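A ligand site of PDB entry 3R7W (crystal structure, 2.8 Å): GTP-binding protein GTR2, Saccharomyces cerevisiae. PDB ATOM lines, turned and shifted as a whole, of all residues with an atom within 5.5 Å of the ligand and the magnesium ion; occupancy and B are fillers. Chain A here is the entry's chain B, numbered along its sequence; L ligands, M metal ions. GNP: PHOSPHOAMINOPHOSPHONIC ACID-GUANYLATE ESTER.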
ATOM      1  N   VAL A   7      -8.478 -12.940  23.449  1.00  0.00           N
ATOM      2  CA  VAL A   7      -9.143 -14.077  24.076  1.00  0.00           C
ATOM      3  C   VAL A   7      -9.567 -15.076  22.997  1.00  0.00           C
ATOM      4  O   VAL A   7     -10.205 -14.708  22.028  1.00  0.00           O
ATOM      5  CB  VAL A   7     -10.361 -13.653  24.922  1.00  0.00           C
ATOM      6  CG1 VAL A   7      -9.898 -12.861  26.135  1.00  0.00           C
ATOM      7  CG2 VAL A   7     -11.343 -12.836  24.077  1.00  0.00           C
ATOM      8  N   ARG A   8      -9.181 -16.343  23.198  1.00  0.00           N
ATOM      9  CA  ARG A   8      -9.441 -17.433  22.248  1.00  0.00           C
ATOM     10  C   ARG A   8     -10.481 -17.170  21.139  1.00  0.00           C
ATOM     11  O   ARG A   8     -11.556 -16.618  21.395  1.00  0.00           O
ATOM     12  CB  ARG A   8      -9.778 -18.721  23.017  1.00  0.00           C
ATOM     13  CG  ARG A   8     -10.262 -19.884  22.142  1.00  0.00           C
ATOM     14  CD  ARG A   8     -10.481 -21.169  22.953  1.00  0.00           C
ATOM     15  NE  ARG A   8     -11.489 -21.018  24.000  1.00  0.00           N
ATOM     16  CZ  ARG A   8     -11.745 -21.936  24.931  1.00  0.00           C
ATOM     17  NH1 ARG A   8     -11.078 -23.079  24.940  1.00  0.00           N
ATOM     18  NH2 ARG A   8     -12.671 -21.701  25.850  1.00  0.00           N
ATOM     19  N   ARG A   9     -10.153 -17.583  19.922  1.00  0.00           N
ATOM     20  CA  ARG A   9     -11.038 -17.468  18.750  1.00  0.00           C
ATOM     21  C   ARG A   9     -11.222 -16.047  18.188  1.00  0.00           C
ATOM     22  O   ARG A   9     -11.939 -15.843  17.214  1.00  0.00           O
ATOM     23  CB  ARG A   9     -12.393 -18.128  19.021  1.00  0.00           C
ATOM     24  CG  ARG A   9     -12.305 -19.617  19.340  1.00  0.00           C
ATOM     25  CD  ARG A   9     -11.385 -20.356  18.368  1.00  0.00           C
ATOM     26  NE  ARG A   9     -12.045 -20.740  17.120  1.00  0.00           N
ATOM     27  CZ  ARG A   9     -11.440 -21.378  16.115  1.00  0.00           C
ATOM     28  NH1 ARG A   9     -10.155 -21.703  16.210  1.00  0.00           N
ATOM     29  NH2 ARG A   9     -12.119 -21.687  15.024  1.00  0.00           N
ATOM     30  N   CYS A  10     -10.557 -15.057  18.794  1.00  0.00           N
ATOM     31  CA  CYS A  10     -10.696 -13.673  18.366  1.00  0.00           C
ATOM     32  C   CYS A  10     -10.204 -13.451  16.935  1.00  0.00           C
ATOM     33  O   CYS A  10     -10.986 -13.076  16.041  1.00  0.00           O
ATOM     34  CB  CYS A  10      -9.985 -12.715  19.336  1.00  0.00           C
ATOM     35  SG  CYS A  10      -8.282 -13.187  19.710  1.00  0.00           S
ATOM     36  N   GLY A  11      -8.906 -13.673  16.724  1.00  0.00           N
ATOM     37  CA  GLY A  11      -8.308 -13.501  15.415  1.00  0.00           C
ATOM     38  C   GLY A  11      -6.797 -13.351  15.435  1.00  0.00           C
ATOM     39  O   GLY A  11      -6.203 -13.021  14.413  1.00  0.00           O
ATOM     40  N   LYS A  12      -6.182 -13.599  16.579  1.00  0.00           N
ATOM     41  CA  LYS A  12      -4.739 -13.396  16.747  1.00  0.00           C
ATOM     42  C   LYS A  12      -3.819 -14.269  15.859  1.00  0.00           C
ATOM     43  O   LYS A  12      -2.705 -13.847  15.506  1.00  0.00           O
ATOM     44  CB  LYS A  12      -4.339 -13.518  18.241  1.00  0.00           C
ATOM     45  CG  LYS A  12      -4.553 -14.891  18.857  1.00  0.00           C
ATOM     46  CD  LYS A  12      -3.942 -15.014  20.247  1.00  0.00           C
ATOM     47  CE  LYS A  12      -4.802 -14.337  21.295  1.00  0.00           C
ATOM     48  NZ  LYS A  12      -4.144 -14.340  22.633  1.00  0.00           N
ATOM     49  N   SER A  13      -4.268 -15.468  15.487  1.00  0.00           N
ATOM     50  CA  SER A  13      -3.423 -16.391  14.727  1.00  0.00           C
ATOM     51  C   SER A  13      -3.791 -16.483  13.244  1.00  0.00           C
ATOM     52  O   SER A  13      -2.942 -16.811  12.414  1.00  0.00           O
ATOM     53  CB  SER A  13      -3.468 -17.792  15.357  1.00  0.00           C
ATOM     54  OG  SER A  13      -2.486 -18.633  14.789  1.00  0.00           O
ATOM     55  N   SER A  14      -5.050 -16.209  12.921  1.00  0.00           N
ATOM     56  CA  SER A  14      -5.516 -16.165  11.531  1.00  0.00           C
ATOM     57  C   SER A  14      -4.851 -15.011  10.782  1.00  0.00           C
ATOM     58  O   SER A  14      -4.509 -15.135   9.600  1.00  0.00           O
ATOM     59  CB  SER A  14      -7.031 -15.991  11.463  1.00  0.00           C
ATOM     60  OG  SER A  14      -7.714 -17.175  11.833  1.00  0.00           O
ATOM     61  N   ILE A  15      -4.693 -13.890  11.470  1.00  0.00           N
ATOM     62  CA  ILE A  15      -4.046 -12.720  10.897  1.00  0.00           C
ATOM     63  C   ILE A  15      -2.531 -12.829  11.040  1.00  0.00           C
ATOM     64  O   ILE A  15      -1.788 -12.094  10.404  1.00  0.00           O
ATOM     65  CB  ILE A  15      -4.531 -11.422  11.548  1.00  0.00           C
ATOM     66  CG1 ILE A  15      -4.057 -11.321  12.997  1.00  0.00           C
ATOM     67  CG2 ILE A  15      -6.048 -11.349  11.501  1.00  0.00           C
ATOM     68  CD1 ILE A  15      -4.776 -10.247  13.792  1.00  0.00           C
ATOM     69  N   THR A  28      -8.582 -20.115   7.026  1.00  0.00           N
ATOM     70  CA  THR A  28      -8.484 -19.775   8.447  1.00  0.00           C
ATOM     71  C   THR A  28      -9.810 -19.884   9.206  1.00  0.00           C
ATOM     72  O   THR A  28      -9.836 -19.781  10.438  1.00  0.00           O
ATOM     73  CB  THR A  28      -7.907 -18.344   8.661  1.00  0.00           C
ATOM     74  OG1 THR A  28      -8.671 -17.394   7.912  1.00  0.00           O
ATOM     75  CG2 THR A  28      -6.457 -18.272   8.238  1.00  0.00           C
ATOM     76  N   LEU A  29     -10.915 -20.072   8.475  1.00  0.00           N
ATOM     77  CA  LEU A  29     -12.235 -20.220   9.099  1.00  0.00           C
ATOM     78  C   LEU A  29     -12.442 -21.573   9.782  1.00  0.00           C
ATOM     79  O   LEU A  29     -13.485 -21.825  10.380  1.00  0.00           O
ATOM     80  CB  LEU A  29     -13.366 -19.932   8.096  1.00  0.00           C
ATOM     81  CG  LEU A  29     -14.066 -18.575   8.223  1.00  0.00           C
ATOM     82  CD1 LEU A  29     -13.113 -17.427   7.849  1.00  0.00           C
ATOM     83  CD2 LEU A  29     -15.328 -18.497   7.382  1.00  0.00           C
ATOM     84  N   TYR A  30     -11.429 -22.431   9.711  1.00  0.00           N
ATOM     85  CA  TYR A  30     -11.465 -23.745  10.345  1.00  0.00           C
ATOM     86  C   TYR A  30     -10.126 -24.118  10.997  1.00  0.00           C
ATOM     87  O   TYR A  30      -9.924 -25.268  11.388  1.00  0.00           O
ATOM     88  CB  TYR A  30     -11.904 -24.836   9.359  1.00  0.00           C
ATOM     89  CG  TYR A  30     -13.401 -25.093   9.329  1.00  0.00           C
ATOM     90  CD1 TYR A  30     -14.007 -25.871  10.312  1.00  0.00           C
ATOM     91  CD2 TYR A  30     -14.202 -24.554   8.322  1.00  0.00           C
ATOM     92  CE1 TYR A  30     -15.373 -26.097  10.302  1.00  0.00           C
ATOM     93  CE2 TYR A  30     -15.569 -24.784   8.302  1.00  0.00           C
ATOM     94  CZ  TYR A  30     -16.145 -25.554   9.291  1.00  0.00           C
ATOM     95  OH  TYR A  30     -17.499 -25.788   9.282  1.00  0.00           O
ATOM     96  N   LEU A  31      -9.224 -23.136  11.099  1.00  0.00           N
ATOM     97  CA  LEU A  31      -7.938 -23.348  11.759  1.00  0.00           C
ATOM     98  C   LEU A  31      -8.143 -23.856  13.188  1.00  0.00           C
ATOM     99  O   LEU A  31      -9.241 -23.772  13.739  1.00  0.00           O
ATOM    100  CB  LEU A  31      -7.094 -22.070  11.754  1.00  0.00           C
ATOM    101  CG  LEU A  31      -5.580 -22.212  11.928  1.00  0.00           C
ATOM    102  CD1 LEU A  31      -4.949 -22.782  10.668  1.00  0.00           C
ATOM    103  CD2 LEU A  31      -4.938 -20.886  12.285  1.00  0.00           C
ATOM    104  N   GLU A  32      -7.073 -24.390  13.789  1.00  0.00           N
ATOM    105  CA  GLU A  32      -7.151 -25.048  15.095  1.00  0.00           C
ATOM    106  C   GLU A  32      -7.110 -24.103  16.301  1.00  0.00           C
ATOM    107  O   GLU A  32      -8.040 -23.310  16.531  1.00  0.00           O
ATOM    108  CB  GLU A  32      -6.067 -26.131  15.225  1.00  0.00           C
ATOM    109  CG  GLU A  32      -5.011 -26.110  14.119  1.00  0.00           C
ATOM    110  CD  GLU A  32      -4.218 -24.812  14.071  1.00  0.00           C
ATOM    111  OE1 GLU A  32      -4.216 -24.073  15.071  1.00  0.00           O
ATOM    112  OE2 GLU A  32      -3.600 -24.529  13.019  1.00  0.00           O
ATOM    113  N   SER A  33      -6.029 -24.192  17.078  1.00  0.00           N
ATOM    114  CA  SER A  33      -5.904 -23.478  18.348  1.00  0.00           C
ATOM    115  C   SER A  33      -4.448 -23.520  18.864  1.00  0.00           C
ATOM    116  O   SER A  33      -4.044 -24.500  19.489  1.00  0.00           O
ATOM    117  CB  SER A  33      -6.861 -24.105  19.381  1.00  0.00           C
ATOM    118  OG  SER A  33      -7.015 -23.278  20.526  1.00  0.00           O
ATOM    119  N   THR A  34      -3.682 -22.463  18.588  1.00  0.00           N
ATOM    120  CA  THR A  34      -2.254 -22.416  18.922  1.00  0.00           C
ATOM    121  C   THR A  34      -1.964 -21.969  20.365  1.00  0.00           C
ATOM    122  O   THR A  34      -1.793 -20.777  20.640  1.00  0.00           O
ATOM    123  CB  THR A  34      -1.466 -21.488  17.938  1.00  0.00           C
ATOM    124  OG1 THR A  34      -2.111 -21.444  16.660  1.00  0.00           O
ATOM    125  CG2 THR A  34      -0.022 -21.966  17.771  1.00  0.00           C
ATOM    126  N   SER A  35      -1.908 -22.939  21.282  1.00  0.00           N
ATOM    127  CA  SER A  35      -1.670 -22.646  22.704  1.00  0.00           C
ATOM    128  C   SER A  35      -0.225 -22.254  23.012  1.00  0.00           C
ATOM    129  O   SER A  35       0.016 -21.272  23.714  1.00  0.00           O
ATOM    130  CB  SER A  35      -2.131 -23.818  23.586  1.00  0.00           C
ATOM    131  OG  SER A  35      -1.452 -25.017  23.253  1.00  0.00           O
ATOM    132  N   GLU A  52       2.860 -14.629  19.755  1.00  0.00           N
ATOM    133  CA  GLU A  52       1.424 -14.626  19.849  1.00  0.00           C
ATOM    134  C   GLU A  52       1.004 -15.531  21.001  1.00  0.00           C
ATOM    135  O   GLU A  52       0.776 -16.726  20.827  1.00  0.00           O
ATOM    136  CB  GLU A  52       0.816 -15.087  18.525  1.00  0.00           C
ATOM    137  CG  GLU A  52      -0.637 -15.488  18.588  1.00  0.00           C
ATOM    138  CD  GLU A  52      -0.807 -16.953  18.324  1.00  0.00           C
ATOM    139  OE1 GLU A  52      -1.964 -17.410  18.260  1.00  0.00           O
ATOM    140  OE2 GLU A  52       0.210 -17.644  18.170  1.00  0.00           O
ATOM    141  N   PRO A  54      -1.172 -17.352  23.826  1.00  0.00           N
ATOM    142  CA  PRO A  54      -2.514 -17.955  23.888  1.00  0.00           C
ATOM    143  C   PRO A  54      -3.442 -17.121  24.758  1.00  0.00           C
ATOM    144  O   PRO A  54      -3.093 -16.805  25.899  1.00  0.00           O
ATOM    145  CB  PRO A  54      -2.254 -19.311  24.549  1.00  0.00           C
ATOM    146  CG  PRO A  54      -0.953 -19.125  25.293  1.00  0.00           C
ATOM    147  CD  PRO A  54      -0.146 -18.227  24.411  1.00  0.00           C
ATOM    148  N   GLY A  55      -4.616 -16.774  24.235  1.00  0.00           N
ATOM    149  CA  GLY A  55      -5.477 -15.785  24.871  1.00  0.00           C
ATOM    150  C   GLY A  55      -6.320 -16.207  26.060  1.00  0.00           C
ATOM    151  O   GLY A  55      -7.538 -16.391  25.918  1.00  0.00           O
ATOM    152  N   ASP A  81     -12.169  -9.540  19.205  1.00  0.00           N
ATOM    153  CA  ASP A  81     -13.267  -9.978  18.342  1.00  0.00           C
ATOM    154  C   ASP A  81     -14.479  -9.020  18.337  1.00  0.00           C
ATOM    155  O   ASP A  81     -14.491  -7.996  19.018  1.00  0.00           O
ATOM    156  CB  ASP A  81     -13.713 -11.390  18.719  1.00  0.00           C
ATOM    157  CG  ASP A  81     -14.222 -12.196  17.525  1.00  0.00           C
ATOM    158  OD1 ASP A  81     -15.265 -11.819  16.949  1.00  0.00           O
ATOM    159  OD2 ASP A  81     -13.576 -13.201  17.156  1.00  0.00           O
ATOM    160  N   HIS A 114     -11.029  -6.070  15.587  1.00  0.00           N
ATOM    161  CA  HIS A 114     -11.024  -7.104  14.552  1.00  0.00           C
ATOM    162  C   HIS A 114     -12.368  -7.761  14.179  1.00  0.00           C
ATOM    163  O   HIS A 114     -13.382  -7.571  14.858  1.00  0.00           O
ATOM    164  CB  HIS A 114     -10.047  -8.201  14.990  1.00  0.00           C
ATOM    165  CG  HIS A 114      -9.850  -9.279  13.972  1.00  0.00           C
ATOM    166  ND1 HIS A 114      -8.846  -9.230  13.031  1.00  0.00           N
ATOM    167  CD2 HIS A 114     -10.518 -10.432  13.753  1.00  0.00           C
ATOM    168  CE1 HIS A 114      -8.907 -10.313  12.269  1.00  0.00           C
ATOM    169  NE2 HIS A 114      -9.923 -11.056  12.692  1.00  0.00           N
ATOM    170  N   LYS A 115     -12.354  -8.540  13.106  1.00  0.00           N
ATOM    171  CA  LYS A 115     -13.518  -9.312  12.658  1.00  0.00           C
ATOM    172  C   LYS A 115     -14.678  -8.386  12.258  1.00  0.00           C
ATOM    173  O   LYS A 115     -15.843  -8.703  12.499  1.00  0.00           O
ATOM    174  CB  LYS A 115     -13.953 -10.325  13.740  1.00  0.00           C
ATOM    175  CG  LYS A 115     -14.765 -11.548  13.231  1.00  0.00           C
ATOM    176  CD  LYS A 115     -16.292 -11.355  13.379  1.00  0.00           C
ATOM    177  CE  LYS A 115     -17.091 -12.580  12.889  1.00  0.00           C
ATOM    178  NZ  LYS A 115     -18.562 -12.313  12.788  1.00  0.00           N
ATOM    179  N   VAL A 116     -14.347  -7.253  11.653  1.00  0.00           N
ATOM    180  CA  VAL A 116     -15.345  -6.274  11.222  1.00  0.00           C
ATOM    181  C   VAL A 116     -15.862  -6.546   9.799  1.00  0.00           C
ATOM    182  O   VAL A 116     -16.125  -5.611   9.038  1.00  0.00           O
ATOM    183  CB  VAL A 116     -14.799  -4.821  11.317  1.00  0.00           C
ATOM    184  CG1 VAL A 116     -15.886  -3.793  11.036  1.00  0.00           C
ATOM    185  CG2 VAL A 116     -14.207  -4.565  12.674  1.00  0.00           C
ATOM    186  N   ASP A 117     -16.002  -7.820   9.441  1.00  0.00           N
ATOM    187  CA  ASP A 117     -16.421  -8.211   8.089  1.00  0.00           C
ATOM    188  C   ASP A 117     -17.723  -7.565   7.621  1.00  0.00           C
ATOM    189  O   ASP A 117     -17.988  -6.389   7.901  1.00  0.00           O
ATOM    190  CB  ASP A 117     -16.542  -9.729   7.974  1.00  0.00           C
ATOM    191  CG  ASP A 117     -15.219 -10.430   8.171  1.00  0.00           C
ATOM    192  OD1 ASP A 117     -14.382  -9.913   8.930  1.00  0.00           O
ATOM    193  OD2 ASP A 117     -15.028 -11.498   7.550  1.00  0.00           O
ATOM    194  N   THR A 154      -9.368  -3.810  11.591  1.00  0.00           N
ATOM    195  CA  THR A 154      -8.960  -5.040  10.894  1.00  0.00           C
ATOM    196  C   THR A 154     -10.136  -5.927  10.462  1.00  0.00           C
ATOM    197  O   THR A 154     -11.214  -5.870  11.051  1.00  0.00           O
ATOM    198  CB  THR A 154      -7.972  -5.886  11.748  1.00  0.00           C
ATOM    199  OG1 THR A 154      -8.218  -5.660  13.142  1.00  0.00           O
ATOM    200  CG2 THR A 154      -6.527  -5.525  11.446  1.00  0.00           C
ATOM    201  N   SER A 155      -9.924  -6.763   9.430  1.00  0.00           N
ATOM    202  CA  SER A 155     -10.980  -7.609   8.878  1.00  0.00           C
ATOM    203  C   SER A 155     -10.489  -8.841   8.122  1.00  0.00           C
ATOM    204  O   SER A 155     -11.297  -9.508   7.481  1.00  0.00           O
ATOM    205  CB  SER A 155     -11.881  -6.802   7.945  1.00  0.00           C
ATOM    206  OG  SER A 155     -12.175  -5.522   8.489  1.00  0.00           O
ATOM    207  N   ILE A 156      -9.191  -9.140   8.187  1.00  0.00           N
ATOM    208  CA  ILE A 156      -8.563 -10.339   7.565  1.00  0.00           C
ATOM    209  C   ILE A 156      -8.998 -10.694   6.129  1.00  0.00           C
ATOM    210  O   ILE A 156      -8.375 -11.543   5.472  1.00  0.00           O
ATOM    211  CB  ILE A 156      -8.638 -11.611   8.473  1.00  0.00           C
ATOM    212  CG1 ILE A 156      -7.308 -12.381   8.429  1.00  0.00           C
ATOM    213  CG2 ILE A 156      -9.788 -12.517   8.065  1.00  0.00           C
ATOM    214  CD1 ILE A 156      -7.426 -13.838   8.842  1.00  0.00           C
ATOM    215  N   PHE A 157     -10.065 -10.059   5.653  1.00  0.00           N
ATOM    216  CA  PHE A 157     -10.586 -10.234   4.306  1.00  0.00           C
ATOM    217  C   PHE A 157     -10.517  -8.890   3.576  1.00  0.00           C
ATOM    218  O   PHE A 157     -10.464  -8.830   2.342  1.00  0.00           O
ATOM    219  CB  PHE A 157     -12.036 -10.749   4.341  1.00  0.00           C
ATOM    220  CG  PHE A 157     -12.173 -12.207   4.692  1.00  0.00           C
ATOM    221  CD1 PHE A 157     -12.147 -13.189   3.713  1.00  0.00           C
ATOM    222  CD2 PHE A 157     -12.368 -12.607   6.013  1.00  0.00           C
ATOM    223  CE1 PHE A 157     -12.305 -14.520   4.038  1.00  0.00           C
ATOM    224  CE2 PHE A 157     -12.514 -13.944   6.349  1.00  0.00           C
ATOM    225  CZ  PHE A 157     -12.482 -14.905   5.363  1.00  0.00           C
HETATM  226  PG  GNP L   1      -6.247 -19.166  20.087  1.00  0.00           P
HETATM  227  O1G GNP L   1      -4.880 -19.014  19.447  1.00  0.00           O
HETATM  228  O2G GNP L   1      -6.654 -20.576  20.449  1.00  0.00           O
HETATM  229  O3G GNP L   1      -6.253 -18.165  21.227  1.00  0.00           O
HETATM  230  N3B GNP L   1      -7.349 -18.709  19.029  1.00  0.00           N
HETATM  231  PB  GNP L   1      -7.041 -17.623  17.914  1.00  0.00           P
HETATM  232  O1B GNP L   1      -7.077 -16.278  18.550  1.00  0.00           O
HETATM  233  O2B GNP L   1      -5.782 -18.065  17.270  1.00  0.00           O
HETATM  234  O3A GNP L   1      -8.165 -17.645  16.860  1.00  0.00           O
HETATM  235  PA  GNP L   1      -7.994 -17.838  15.337  1.00  0.00           P
HETATM  236  O1A GNP L   1      -7.168 -16.710  14.834  1.00  0.00           O
HETATM  237  O2A GNP L   1      -7.531 -19.209  15.027  1.00  0.00           O
HETATM  238  O5' GNP L   1      -9.403 -17.661  14.638  1.00  0.00           O
HETATM  239  C5' GNP L   1     -10.578 -18.191  15.240  1.00  0.00           C
HETATM  240  C4' GNP L   1     -11.811 -17.897  14.392  1.00  0.00           C
HETATM  241  O4' GNP L   1     -11.800 -16.498  14.029  1.00  0.00           O
HETATM  242  C3' GNP L   1     -11.939 -18.697  13.087  1.00  0.00           C
HETATM  243  O3' GNP L   1     -13.243 -19.301  12.978  1.00  0.00           O
HETATM  244  C2' GNP L   1     -11.673 -17.644  11.997  1.00  0.00           C
HETATM  245  O2' GNP L   1     -12.399 -17.864  10.809  1.00  0.00           O
HETATM  246  C1' GNP L   1     -12.226 -16.399  12.692  1.00  0.00           C
HETATM  247  N9  GNP L   1     -11.739 -15.141  12.160  1.00  0.00           N
HETATM  248  C8  GNP L   1     -10.467 -14.627  12.236  1.00  0.00           C
HETATM  249  N7  GNP L   1     -10.369 -13.460  11.674  1.00  0.00           N
HETATM  250  C5  GNP L   1     -11.656 -13.189  11.218  1.00  0.00           C
HETATM  251  C6  GNP L   1     -12.173 -12.063  10.516  1.00  0.00           C
HETATM  252  O6  GNP L   1     -11.586 -11.040  10.163  1.00  0.00           O
HETATM  253  N1  GNP L   1     -13.538 -12.208  10.239  1.00  0.00           N
HETATM  254  C2  GNP L   1     -14.301 -13.287  10.584  1.00  0.00           C
HETATM  255  N2  GNP L   1     -15.593 -13.244  10.220  1.00  0.00           N
HETATM  256  N3  GNP L   1     -13.823 -14.344  11.225  1.00  0.00           N
HETATM  257  C4  GNP L   1     -12.507 -14.217  11.503  1.00  0.00           C
HETATM  258 MG    MG M   1      -3.760 -19.353  17.259  1.00  0.00          MG
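NH1 of Arg 9 is in salt-bridge range of O2A of the ligand (3.8 Å). N of Lys 12 lies close to O1B of the ligand, 3.4 Å away. The side-chain sulfur (SG) of Cys 10 sits at hydrogen-bond distance from an oxygen (O1B) of the ligand, at 3.5 Å. N1 of the ligand lies within hydrogen-bond range of OD1 of Asp 117 (2.8 Å). O of Thr 28 lies close to O2' of the ligand, at 3.2 Å. OG of Ser 14 sits at hydrogen-bond distance from O1A of the ligand (3.1 Å). An oxygen (O1A) of the ligand lies within hydrogen-bond range of the backbone NH of Ser 14 (2.9 Å). The side-chain hydroxyl (OG) of Ser 33 sits at hydrogen-bond distance from an oxygen (O2G) of the ligand (2.7 Å). The backbone NH (N) of Ser 13 lies within hydrogen-bond range of an oxygen (O1A) of the ligand, at 3.2 Å. A nitrogen (N7) of the ligand sits at hydrogen-bond distance from a ring nitrogen (NE2) of His 114, at 2.6 Å.
CB of Ser 13 touches the magnesium ion, at 2.5 Å. The nearest printed residue that does not touch the magnesium ion is Ser 33 (4.5 Å).
The magnesium ion is bound by an oxygen (O2B) of the ligand (2.4 Å) and an oxygen (O1G) of the ligand (2.5 Å). Slightly farther from the magnesium ion lies OG1 of Thr 34 (2.7 Å). Slightly farther from the magnesium ion lies the side-chain carboxylate (OE1) of Glu 52 (2.8 Å).
The backbone NH of Arg 8 lies within hydrogen-bond range of the backbone carbonyl oxygen of Gly 55. O of Glu 32 sits at hydrogen-bond distance from NH1 of Arg 9, at 2.7 Å. The backbone carbonyl oxygen (O) of Val 7 sits close to the side-chain sulfur (SG) of Cys 10 (3.4 Å). OG of Ser 13 is in hydrogen-bond range of OG1 of Thr 34 (3.4 Å). The guanidinium group of Arg 9 lies within hydrogen-bond range of the backbone carbonyl oxygen of Leu 31. N of Lys 12 lies within hydrogen-bond range of SG of Cys 10 (3.8 Å).
An oxygen (O6) of the ligand sits close to the backbone carbonyl oxygen of Ser 155, 3.1 Å away. Merely in contact with the ligand: Arg 8, Gly 11, Leu 29, Gly 55, Lys 115 and Ile 156. Hydrophobic or aromatic side chains within 4 Å of the ligand: Leu 29, His 114 and Ile 156. 18 residues have an atom within 4 Å of the ligand: Arg 8, Arg 9, Cys 10, Gly 11, Lys 12, Ser 13, Ser 14, Thr 28, Leu 29, Ser 33, Thr 34, Glu 52, Gly 55, His 114, Lys 115, Asp 117, Ser 155 and Ile 156. The nearest printed residue that does not touch the ligand is Leu 31 (4.1 Å).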
